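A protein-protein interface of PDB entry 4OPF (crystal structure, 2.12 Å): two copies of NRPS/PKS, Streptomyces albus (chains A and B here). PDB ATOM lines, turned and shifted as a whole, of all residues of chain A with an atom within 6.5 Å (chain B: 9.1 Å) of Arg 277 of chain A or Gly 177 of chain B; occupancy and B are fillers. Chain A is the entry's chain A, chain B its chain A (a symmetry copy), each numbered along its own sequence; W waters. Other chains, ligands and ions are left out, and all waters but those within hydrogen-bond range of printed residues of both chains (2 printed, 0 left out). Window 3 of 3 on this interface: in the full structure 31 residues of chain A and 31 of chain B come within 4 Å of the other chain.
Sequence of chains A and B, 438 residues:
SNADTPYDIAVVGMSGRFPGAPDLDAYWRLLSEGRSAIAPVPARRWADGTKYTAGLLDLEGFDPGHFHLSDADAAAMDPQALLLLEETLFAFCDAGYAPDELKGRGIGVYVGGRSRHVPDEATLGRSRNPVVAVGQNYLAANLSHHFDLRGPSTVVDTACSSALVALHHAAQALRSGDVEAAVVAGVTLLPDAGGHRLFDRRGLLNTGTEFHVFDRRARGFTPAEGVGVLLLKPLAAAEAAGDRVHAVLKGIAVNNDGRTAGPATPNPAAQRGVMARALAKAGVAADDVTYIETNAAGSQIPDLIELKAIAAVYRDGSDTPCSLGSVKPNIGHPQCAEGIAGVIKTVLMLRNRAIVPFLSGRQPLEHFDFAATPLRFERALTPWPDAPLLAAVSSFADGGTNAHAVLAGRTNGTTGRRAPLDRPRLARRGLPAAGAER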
ATOM      1  N   GLN A 172     -18.755  20.079 -28.104  1.00  0.00           N
ATOM      2  CA  GLN A 172     -20.008  20.335 -27.366  1.00  0.00           C
ATOM      3  C   GLN A 172     -20.521  19.058 -26.758  1.00  0.00           C
ATOM      4  O   GLN A 172     -20.962  19.040 -25.615  1.00  0.00           O
ATOM      5  CB  GLN A 172     -21.070  20.872 -28.274  1.00  0.00           C
ATOM      6  CG  GLN A 172     -20.649  22.058 -29.135  1.00  0.00           C
ATOM      7  CD  GLN A 172     -21.315  23.336 -28.778  1.00  0.00           C
ATOM      8  OE1 GLN A 172     -22.461  23.562 -29.137  1.00  0.00           O
ATOM      9  NE2 GLN A 172     -20.589  24.213 -28.080  1.00  0.00           N
ATOM     10  N   GLY A 251     -10.205  25.320 -26.999  1.00  0.00           N
ATOM     11  CA  GLY A 251     -11.436  26.034 -27.354  1.00  0.00           C
ATOM     12  C   GLY A 251     -11.646  26.006 -28.854  1.00  0.00           C
ATOM     13  O   GLY A 251     -10.702  25.908 -29.645  1.00  0.00           O
ATOM     14  N   ILE A 252     -12.897  25.950 -29.242  1.00  0.00           N
ATOM     15  CA  ILE A 252     -13.306  25.983 -30.642  1.00  0.00           C
ATOM     16  C   ILE A 252     -14.602  26.759 -30.766  1.00  0.00           C
ATOM     17  O   ILE A 252     -15.456  26.651 -29.880  1.00  0.00           O
ATOM     18  CB  ILE A 252     -13.369  24.595 -31.260  1.00  0.00           C
ATOM     19  CG1 ILE A 252     -13.877  24.714 -32.682  1.00  0.00           C
ATOM     20  CG2 ILE A 252     -14.266  23.683 -30.439  1.00  0.00           C
ATOM     21  CD1 ILE A 252     -13.541  23.547 -33.493  1.00  0.00           C
ATOM     22  N   ALA A 253     -14.723  27.591 -31.806  1.00  0.00           N
ATOM     23  CA  ALA A 253     -15.904  28.378 -32.027  1.00  0.00           C
ATOM     24  C   ALA A 253     -16.261  28.358 -33.491  1.00  0.00           C
ATOM     25  O   ALA A 253     -15.381  28.177 -34.331  1.00  0.00           O
ATOM     26  CB  ALA A 253     -15.680  29.795 -31.615  1.00  0.00           C
ATOM     27  N   VAL A 254     -17.561  28.522 -33.770  1.00  0.00           N
ATOM     28  CA  VAL A 254     -18.115  28.524 -35.107  1.00  0.00           C
ATOM     29  C   VAL A 254     -19.077  29.682 -35.180  1.00  0.00           C
ATOM     30  O   VAL A 254     -19.823  29.918 -34.252  1.00  0.00           O
ATOM     31  CB  VAL A 254     -18.824  27.216 -35.403  1.00  0.00           C
ATOM     32  CG1 VAL A 254     -19.589  27.251 -36.741  1.00  0.00           C
ATOM     33  CG2 VAL A 254     -17.819  26.090 -35.421  1.00  0.00           C
ATOM     34  N   ARG A 272     -13.102  38.272 -37.045  1.00  0.00           N
ATOM     35  CA  ARG A 272     -12.660  38.697 -35.730  1.00  0.00           C
ATOM     36  C   ARG A 272     -13.447  38.004 -34.627  1.00  0.00           C
ATOM     37  O   ARG A 272     -12.860  37.473 -33.708  1.00  0.00           O
ATOM     38  CB  ARG A 272     -12.757  40.203 -35.564  1.00  0.00           C
ATOM     39  CG  ARG A 272     -11.799  40.989 -36.440  1.00  0.00           C
ATOM     40  CD  ARG A 272     -11.827  42.508 -36.171  1.00  0.00           C
ATOM     41  NE  ARG A 272     -12.988  43.197 -36.682  1.00  0.00           N
ATOM     42  CZ  ARG A 272     -13.116  43.703 -37.907  1.00  0.00           C
ATOM     43  NH1 ARG A 272     -14.235  44.309 -38.271  1.00  0.00           N
ATOM     44  NH2 ARG A 272     -12.150  43.612 -38.801  1.00  0.00           N
ATOM     45  N   GLY A 273     -14.766  37.980 -34.744  1.00  0.00           N
ATOM     46  CA  GLY A 273     -15.606  37.446 -33.706  1.00  0.00           C
ATOM     47  C   GLY A 273     -15.347  35.959 -33.430  1.00  0.00           C
ATOM     48  O   GLY A 273     -15.310  35.539 -32.295  1.00  0.00           O
ATOM     49  N   VAL A 274     -15.170  35.147 -34.475  1.00  0.00           N
ATOM     50  CA  VAL A 274     -15.020  33.714 -34.260  1.00  0.00           C
ATOM     51  C   VAL A 274     -13.676  33.460 -33.603  1.00  0.00           C
ATOM     52  O   VAL A 274     -13.540  32.594 -32.731  1.00  0.00           O
ATOM     53  CB  VAL A 274     -15.200  32.907 -35.543  1.00  0.00           C
ATOM     54  CG1 VAL A 274     -13.950  32.940 -36.413  1.00  0.00           C
ATOM     55  CG2 VAL A 274     -15.512  31.497 -35.181  1.00  0.00           C
ATOM     56  N   MET A 275     -12.684  34.248 -33.960  1.00  0.00           N
ATOM     57  CA  MET A 275     -11.364  34.047 -33.337  1.00  0.00           C
ATOM     58  C   MET A 275     -11.390  34.518 -31.889  1.00  0.00           C
ATOM     59  O   MET A 275     -10.884  33.818 -31.013  1.00  0.00           O
ATOM     60  CB  MET A 275     -10.244  34.759 -34.073  1.00  0.00           C
ATOM     61  CG  MET A 275     -10.030  34.215 -35.495  1.00  0.00           C
ATOM     62  SD  MET A 275      -8.376  34.943 -36.310  1.00  0.00           S
ATOM     63  CE  MET A 275      -9.119  36.628 -36.856  1.00  0.00           C
ATOM     64  N   ALA A 276     -11.959  35.685 -31.625  1.00  0.00           N
ATOM     65  CA  ALA A 276     -12.088  36.159 -30.242  1.00  0.00           C
ATOM     66  C   ALA A 276     -12.912  35.228 -29.378  1.00  0.00           C
ATOM     67  O   ALA A 276     -12.588  34.995 -28.219  1.00  0.00           O
ATOM     68  CB  ALA A 276     -12.689  37.571 -30.219  1.00  0.00           C
ATOM     69  N   ARG A 277     -13.973  34.634 -29.922  1.00  0.00           N
ATOM     70  CA  ARG A 277     -14.741  33.653 -29.174  1.00  0.00           C
ATOM     71  C   ARG A 277     -13.961  32.403 -28.838  1.00  0.00           C
ATOM     72  O   ARG A 277     -14.051  31.869 -27.719  1.00  0.00           O
ATOM     73  CB  ARG A 277     -16.035  33.322 -29.956  1.00  0.00           C
ATOM     74  CG  ARG A 277     -16.955  32.319 -29.301  1.00  0.00           C
ATOM     75  CD  ARG A 277     -17.598  32.834 -27.982  1.00  0.00           C
ATOM     76  NE  ARG A 277     -18.334  31.701 -27.392  1.00  0.00           N
ATOM     77  CZ  ARG A 277     -18.574  31.528 -26.100  1.00  0.00           C
ATOM     78  NH1 ARG A 277     -19.214  30.429 -25.703  1.00  0.00           N
ATOM     79  NH2 ARG A 277     -18.159  32.436 -25.216  1.00  0.00           N
ATOM     80  N   ALA A 278     -13.215  31.855 -29.780  1.00  0.00           N
ATOM     81  CA  ALA A 278     -12.459  30.631 -29.467  1.00  0.00           C
ATOM     82  C   ALA A 278     -11.430  30.892 -28.383  1.00  0.00           C
ATOM     83  O   ALA A 278     -11.186  30.041 -27.501  1.00  0.00           O
ATOM     84  CB  ALA A 278     -11.746  30.081 -30.683  1.00  0.00           C
ATOM     85  N   LEU A 279     -10.785  32.033 -28.473  1.00  0.00           N
ATOM     86  CA  LEU A 279      -9.840  32.443 -27.415  1.00  0.00           C
ATOM     87  C   LEU A 279     -10.444  32.573 -26.042  1.00  0.00           C
ATOM     88  O   LEU A 279      -9.846  32.102 -25.071  1.00  0.00           O
ATOM     89  CB  LEU A 279      -9.248  33.798 -27.709  1.00  0.00           C
ATOM     90  CG  LEU A 279      -8.074  33.833 -28.628  1.00  0.00           C
ATOM     91  CD1 LEU A 279      -7.645  35.310 -28.595  1.00  0.00           C
ATOM     92  CD2 LEU A 279      -6.898  32.955 -28.150  1.00  0.00           C
ATOM     93  N   ALA A 280     -11.603  33.228 -25.950  1.00  0.00           N
ATOM     94  CA  ALA A 280     -12.327  33.302 -24.707  1.00  0.00           C
ATOM     95  C   ALA A 280     -12.677  31.928 -24.155  1.00  0.00           C
ATOM     96  O   ALA A 280     -12.506  31.698 -22.964  1.00  0.00           O
ATOM     97  CB  ALA A 280     -13.595  34.154 -24.869  1.00  0.00           C
ATOM     98  N   LYS A 281     -13.121  30.990 -24.995  1.00  0.00           N
ATOM     99  CA  LYS A 281     -13.484  29.670 -24.508  1.00  0.00           C
ATOM    100  C   LYS A 281     -12.240  28.945 -24.025  1.00  0.00           C
ATOM    101  O   LYS A 281     -12.299  28.143 -23.107  1.00  0.00           O
ATOM    102  CB  LYS A 281     -14.179  28.820 -25.605  1.00  0.00           C
ATOM    103  CG  LYS A 281     -15.587  29.313 -25.968  1.00  0.00           C
ATOM    104  CD  LYS A 281     -16.190  28.627 -27.216  1.00  0.00           C
ATOM    105  CE  LYS A 281     -16.954  27.342 -26.882  1.00  0.00           C
ATOM    106  NZ  LYS A 281     -17.590  26.685 -28.099  1.00  0.00           N
ATOM    107  N   ALA A 282     -11.111  29.216 -24.662  1.00  0.00           N
ATOM    108  CA  ALA A 282      -9.890  28.566 -24.313  1.00  0.00           C
ATOM    109  C   ALA A 282      -9.288  29.076 -22.974  1.00  0.00           C
ATOM    110  O   ALA A 282      -8.485  28.401 -22.364  1.00  0.00           O
ATOM    111  CB  ALA A 282      -8.918  28.822 -25.409  1.00  0.00           C
ATOM    112  N   TYR B   7     -30.664  22.453 -17.847  1.00  0.00           N
ATOM    113  CA  TYR B   7     -30.565  23.752 -18.502  1.00  0.00           C
ATOM    114  C   TYR B   7     -31.853  24.005 -19.322  1.00  0.00           C
ATOM    115  O   TYR B   7     -32.080  23.335 -20.316  1.00  0.00           O
ATOM    116  CB  TYR B   7     -29.315  23.779 -19.407  1.00  0.00           C
ATOM    117  CG  TYR B   7     -29.125  25.104 -20.132  1.00  0.00           C
ATOM    118  CD1 TYR B   7     -28.479  26.167 -19.510  1.00  0.00           C
ATOM    119  CD2 TYR B   7     -29.592  25.292 -21.447  1.00  0.00           C
ATOM    120  CE1 TYR B   7     -28.322  27.391 -20.155  1.00  0.00           C
ATOM    121  CE2 TYR B   7     -29.439  26.514 -22.099  1.00  0.00           C
ATOM    122  CZ  TYR B   7     -28.819  27.551 -21.458  1.00  0.00           C
ATOM    123  OH  TYR B   7     -28.651  28.756 -22.065  1.00  0.00           O
ATOM    124  N   GLY B 106     -26.313  36.899 -32.648  1.00  0.00           N
ATOM    125  CA  GLY B 106     -25.688  35.572 -32.516  1.00  0.00           C
ATOM    126  C   GLY B 106     -26.700  34.452 -32.399  1.00  0.00           C
ATOM    127  O   GLY B 106     -26.830  33.829 -31.362  1.00  0.00           O
ATOM    128  N   TYR B 110     -30.468  25.667 -37.184  1.00  0.00           N
ATOM    129  CA  TYR B 110     -30.298  24.233 -37.192  1.00  0.00           C
ATOM    130  C   TYR B 110     -31.479  23.624 -37.895  1.00  0.00           C
ATOM    131  O   TYR B 110     -32.609  23.717 -37.399  1.00  0.00           O
ATOM    132  CB  TYR B 110     -30.209  23.712 -35.741  1.00  0.00           C
ATOM    133  CG  TYR B 110     -29.075  24.380 -34.987  1.00  0.00           C
ATOM    134  CD1 TYR B 110     -27.773  23.920 -35.074  1.00  0.00           C
ATOM    135  CD2 TYR B 110     -29.283  25.557 -34.327  1.00  0.00           C
ATOM    136  CE1 TYR B 110     -26.729  24.568 -34.396  1.00  0.00           C
ATOM    137  CE2 TYR B 110     -28.264  26.193 -33.654  1.00  0.00           C
ATOM    138  CZ  TYR B 110     -26.993  25.704 -33.704  1.00  0.00           C
ATOM    139  OH  TYR B 110     -25.980  26.382 -33.041  1.00  0.00           O
ATOM    140  N   PRO B 152     -23.795  29.664 -35.621  1.00  0.00           N
ATOM    141  CA  PRO B 152     -23.602  28.522 -36.531  1.00  0.00           C
ATOM    142  C   PRO B 152     -24.844  28.191 -37.331  1.00  0.00           C
ATOM    143  O   PRO B 152     -25.966  28.352 -36.827  1.00  0.00           O
ATOM    144  CB  PRO B 152     -23.222  27.350 -35.588  1.00  0.00           C
ATOM    145  CG  PRO B 152     -22.882  27.982 -34.291  1.00  0.00           C
ATOM    146  CD  PRO B 152     -23.615  29.286 -34.197  1.00  0.00           C
ATOM    147  N   ALA B 170     -28.983  22.589 -31.298  1.00  0.00           N
ATOM    148  CA  ALA B 170     -29.336  23.892 -30.795  1.00  0.00           C
ATOM    149  C   ALA B 170     -29.201  23.955 -29.267  1.00  0.00           C
ATOM    150  O   ALA B 170     -28.642  24.928 -28.713  1.00  0.00           O
ATOM    151  CB  ALA B 170     -30.729  24.268 -31.192  1.00  0.00           C
ATOM    152  N   ALA B 171     -29.716  22.957 -28.586  1.00  0.00           N
ATOM    153  CA  ALA B 171     -29.631  22.932 -27.101  1.00  0.00           C
ATOM    154  C   ALA B 171     -28.178  22.919 -26.615  1.00  0.00           C
ATOM    155  O   ALA B 171     -27.839  23.615 -25.664  1.00  0.00           O
ATOM    156  CB  ALA B 171     -30.337  21.705 -26.583  1.00  0.00           C
ATOM    157  N   GLN B 172     -27.321  22.151 -27.273  1.00  0.00           N
ATOM    158  CA  GLN B 172     -25.895  22.169 -26.896  1.00  0.00           C
ATOM    159  C   GLN B 172     -25.319  23.542 -27.108  1.00  0.00           C
ATOM    160  O   GLN B 172     -24.571  24.045 -26.279  1.00  0.00           O
ATOM    161  CB  GLN B 172     -25.105  21.204 -27.725  1.00  0.00           C
ATOM    162  CG  GLN B 172     -25.671  19.791 -27.795  1.00  0.00           C
ATOM    163  CD  GLN B 172     -24.841  18.768 -27.108  1.00  0.00           C
ATOM    164  OE1 GLN B 172     -23.834  18.325 -27.638  1.00  0.00           O
ATOM    165  NE2 GLN B 172     -25.271  18.357 -25.913  1.00  0.00           N
ATOM    166  N   ALA B 173     -25.708  24.206 -28.217  1.00  0.00           N
ATOM    167  CA  ALA B 173     -25.163  25.511 -28.469  1.00  0.00           C
ATOM    168  C   ALA B 173     -25.634  26.515 -27.439  1.00  0.00           C
ATOM    169  O   ALA B 173     -24.878  27.409 -26.984  1.00  0.00           O
ATOM    170  CB  ALA B 173     -25.498  25.960 -29.899  1.00  0.00           C
ATOM    171  N   LEU B 174     -26.885  26.429 -27.068  1.00  0.00           N
ATOM    172  CA  LEU B 174     -27.416  27.353 -26.094  1.00  0.00           C
ATOM    173  C   LEU B 174     -26.794  27.086 -24.685  1.00  0.00           C
ATOM    174  O   LEU B 174     -26.407  27.998 -23.994  1.00  0.00           O
ATOM    175  CB  LEU B 174     -28.924  27.214 -26.035  1.00  0.00           C
ATOM    176  CG  LEU B 174     -29.705  27.822 -27.187  1.00  0.00           C
ATOM    177  CD1 LEU B 174     -31.092  27.223 -27.214  1.00  0.00           C
ATOM    178  CD2 LEU B 174     -29.813  29.308 -27.021  1.00  0.00           C
ATOM    179  N   ARG B 175     -26.719  25.837 -24.286  1.00  0.00           N
ATOM    180  CA  ARG B 175     -26.133  25.436 -22.981  1.00  0.00           C
ATOM    181  C   ARG B 175     -24.656  25.905 -22.848  1.00  0.00           C
ATOM    182  O   ARG B 175     -24.265  26.372 -21.815  1.00  0.00           O
ATOM    183  CB  ARG B 175     -26.288  23.904 -22.843  1.00  0.00           C
ATOM    184  CG  ARG B 175     -25.768  23.225 -21.574  1.00  0.00           C
ATOM    185  CD  ARG B 175     -25.488  21.702 -21.792  1.00  0.00           C
ATOM    186  NE  ARG B 175     -26.696  20.862 -22.008  1.00  0.00           N
ATOM    187  CZ  ARG B 175     -27.527  20.425 -21.042  1.00  0.00           C
ATOM    188  NH1 ARG B 175     -27.326  20.719 -19.765  1.00  0.00           N
ATOM    189  NH2 ARG B 175     -28.590  19.694 -21.353  1.00  0.00           N
ATOM    190  N   SER B 176     -23.879  25.849 -23.921  1.00  0.00           N
ATOM    191  CA  SER B 176     -22.484  26.245 -23.885  1.00  0.00           C
ATOM    192  C   SER B 176     -22.289  27.748 -24.056  1.00  0.00           C
ATOM    193  O   SER B 176     -21.169  28.242 -23.998  1.00  0.00           O
ATOM    194  CB  SER B 176     -21.719  25.494 -24.978  1.00  0.00           C
ATOM    195  OG  SER B 176     -22.153  25.982 -26.234  1.00  0.00           O
ATOM    196  N   GLY B 177     -23.354  28.509 -24.279  1.00  0.00           N
ATOM    197  CA  GLY B 177     -23.187  29.979 -24.441  1.00  0.00           C
ATOM    198  C   GLY B 177     -22.681  30.357 -25.839  1.00  0.00           C
ATOM    199  O   GLY B 177     -22.335  31.495 -26.075  1.00  0.00           O
ATOM    200  N   ASP B 178     -22.682  29.426 -26.787  1.00  0.00           N
ATOM    201  CA  ASP B 178     -22.254  29.760 -28.152  1.00  0.00           C
ATOM    202  C   ASP B 178     -23.239  30.644 -28.963  1.00  0.00           C
ATOM    203  O   ASP B 178     -22.828  31.376 -29.853  1.00  0.00           O
ATOM    204  CB  ASP B 178     -21.906  28.480 -28.921  1.00  0.00           C
ATOM    205  CG  ASP B 178     -20.530  27.880 -28.504  1.00  0.00           C
ATOM    206  OD1 ASP B 178     -19.761  28.490 -27.679  1.00  0.00           O
ATOM    207  OD2 ASP B 178     -20.213  26.779 -29.016  1.00  0.00           O
ATOM    208  N   VAL B 179     -24.531  30.573 -28.651  1.00  0.00           N
ATOM    209  CA  VAL B 179     -25.564  31.410 -29.281  1.00  0.00           C
ATOM    210  C   VAL B 179     -26.448  31.978 -28.180  1.00  0.00           C
ATOM    211  O   VAL B 179     -26.597  31.356 -27.114  1.00  0.00           O
ATOM    212  CB  VAL B 179     -26.404  30.607 -30.277  1.00  0.00           C
ATOM    213  CG1 VAL B 179     -25.534  30.061 -31.385  1.00  0.00           C
ATOM    214  CG2 VAL B 179     -27.125  29.432 -29.610  1.00  0.00           C
ATOM    215  N   GLU B 180     -27.019  33.125 -28.434  1.00  0.00           N
ATOM    216  CA  GLU B 180     -28.055  33.677 -27.558  1.00  0.00           C
ATOM    217  C   GLU B 180     -29.449  33.132 -27.887  1.00  0.00           C
ATOM    218  O   GLU B 180     -30.367  33.230 -27.069  1.00  0.00           O
ATOM    219  CB  GLU B 180     -28.048  35.206 -27.603  1.00  0.00           C
ATOM    220  CG  GLU B 180     -28.483  35.767 -28.941  1.00  0.00           C
ATOM    221  CD  GLU B 180     -28.938  37.231 -28.907  1.00  0.00           C
ATOM    222  OE1 GLU B 180     -28.067  38.126 -28.849  1.00  0.00           O
ATOM    223  OE2 GLU B 180     -30.182  37.469 -28.998  1.00  0.00           O
ATOM    224  N   ALA B 181     -29.627  32.587 -29.081  1.00  0.00           N
ATOM    225  CA  ALA B 181     -30.911  32.065 -29.465  1.00  0.00           C
ATOM    226  C   ALA B 181     -30.692  31.188 -30.647  1.00  0.00           C
ATOM    227  O   ALA B 181     -29.620  31.212 -31.232  1.00  0.00           O
ATOM    228  CB  ALA B 181     -31.855  33.215 -29.802  1.00  0.00           C
ATOM    229  N   PRO B 234     -32.515  30.697 -23.944  1.00  0.00           N
ATOM    230  CA  PRO B 234     -32.430  30.214 -22.559  1.00  0.00           C
ATOM    231  C   PRO B 234     -33.607  30.784 -21.749  1.00  0.00           C
ATOM    232  O   PRO B 234     -33.986  31.964 -21.937  1.00  0.00           O
ATOM    233  CB  PRO B 234     -31.098  30.822 -22.069  1.00  0.00           C
ATOM    234  CG  PRO B 234     -30.306  31.125 -23.327  1.00  0.00           C
ATOM    235  CD  PRO B 234     -31.376  31.559 -24.299  1.00  0.00           C
HETATM  236  O   HOH W   1     -19.131  28.872 -31.236  1.00  0.00           O
HETATM  237  O   HOH W   2     -19.951  31.404 -30.120  1.00  0.00           O
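Water W2 lies within hydrogen-bond range of O of Asp 178 of chain B (2.9 Å) and NE of Arg 277 of chain A (3.2 Å).
Water W1 lies within hydrogen-bond range of the backbone NH (N) of Val 254 of chain A (3.0 Å) and the side-chain carboxylate (OD2) of Asp 178 of chain B (3.2 Å).
Of the printed residues of chain B, Val 254 of chain A touches Pro 152.
No residue of chain B comes within 4 Å of Ala 276 of chain A.
Printed residues of chain B within 4 Å of Arg 277 of chain A: Ser 176, Gly 177 and Asp 178.
No residue of chain B comes within 4 Å of Ala 278 of chain A.
No residue of chain B comes within 4 Å of Ala 280 of chain A.
Printed residues of chain B within 4 Å of Lys 281 of chain A: Asp 178 (2.8 Å).
Ala 282 of chain A touches none of the printed residues of chain B.
Gly 177 of chain B touches just one residue of chain A: Arg 277.
Ala 181 of chain B touches none of the printed residues of chain A.
The nearest residue of chain B that does not touch Arg 277 of chain A is Val 179 of chain B (6.1 Å).
Of the 17 printed residues of chain B, 6 touch a printed residue of chain A.
Among the printed residues, Asp or Glu carboxylates within 4 Å of a Lys or Arg side-chain nitrogen of the other chain: Arg 277 of chain A with Asp 178 of chain B (2.8 Å) and Lys 281 of chain A with Asp 178 of chain B (2.8 Å).
The side-chain amide oxygen of Gln 172 of chain A lies close to the backbone NH of Ala 173 of chain B, 3.4 Å away.
The side-chain amide nitrogen (NE2) of Gln 172 of chain A lies within hydrogen-bond range of the side-chain hydroxyl (OG) of Ser 176 of chain B, 3.0 Å away.
NE2 of Gln 172 of chain A sits at hydrogen-bond distance from OD2 of Asp 178 of chain B.
The backbone carbonyl oxygen (O) of Ser 176 of chain B lies within hydrogen-bond range of the guanidinium group (NH1) of Arg 277 of chain A, 3.4 Å away.
The guanidinium group of Arg 277 of chain A sits at hydrogen-bond distance from the backbone carbonyl oxygen of Gly 177 of chain B, at 3.3 Å.
The side-chain carboxylate (OD1) of Asp 178 of chain B is in salt-bridge range of the guanidinium group (NH1) of Arg 277 of chain A, 2.8 Å away.
The side-chain amino group (NZ) of Lys 281 of chain A is in salt-bridge range of the side-chain carboxylate (OD2) of Asp 178 of chain B, at 2.8 Å.
Gln 172 of chain A touches its own counterpart, Gln 172 of chain B.
Of the 9 pairs that touch across the chains among the printed residues, 1 has its exchanged pair printed and touching as well.
O of Ile 252 of chain A lies within hydrogen-bond range of NZ of Lys 281 of chain A (2.8 Å).
The backbone carbonyl oxygen (O) of Gln 172 of chain B lies within hydrogen-bond range of the side-chain hydroxyl (OG) of Ser 176 of chain B (3.1 Å).
O of Ala 173 of chain B sits at hydrogen-bond distance from OG of Ser 176 of chain B (3.2 Å).
N of Asp 178 of chain B lies within hydrogen-bond range of O of Ala 173 of chain B, 3.0 Å away.
The side-chain carboxylate (OD2) of Asp 178 of chain B sits close to the side-chain hydroxyl (OG) of Ser 176 of chain B (3.5 Å).
Gln 172 of chain B touches Gln 172 of chain A.
O of Val 254 of chain A touches CG of Pro 152 of chain B (3.6 Å).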
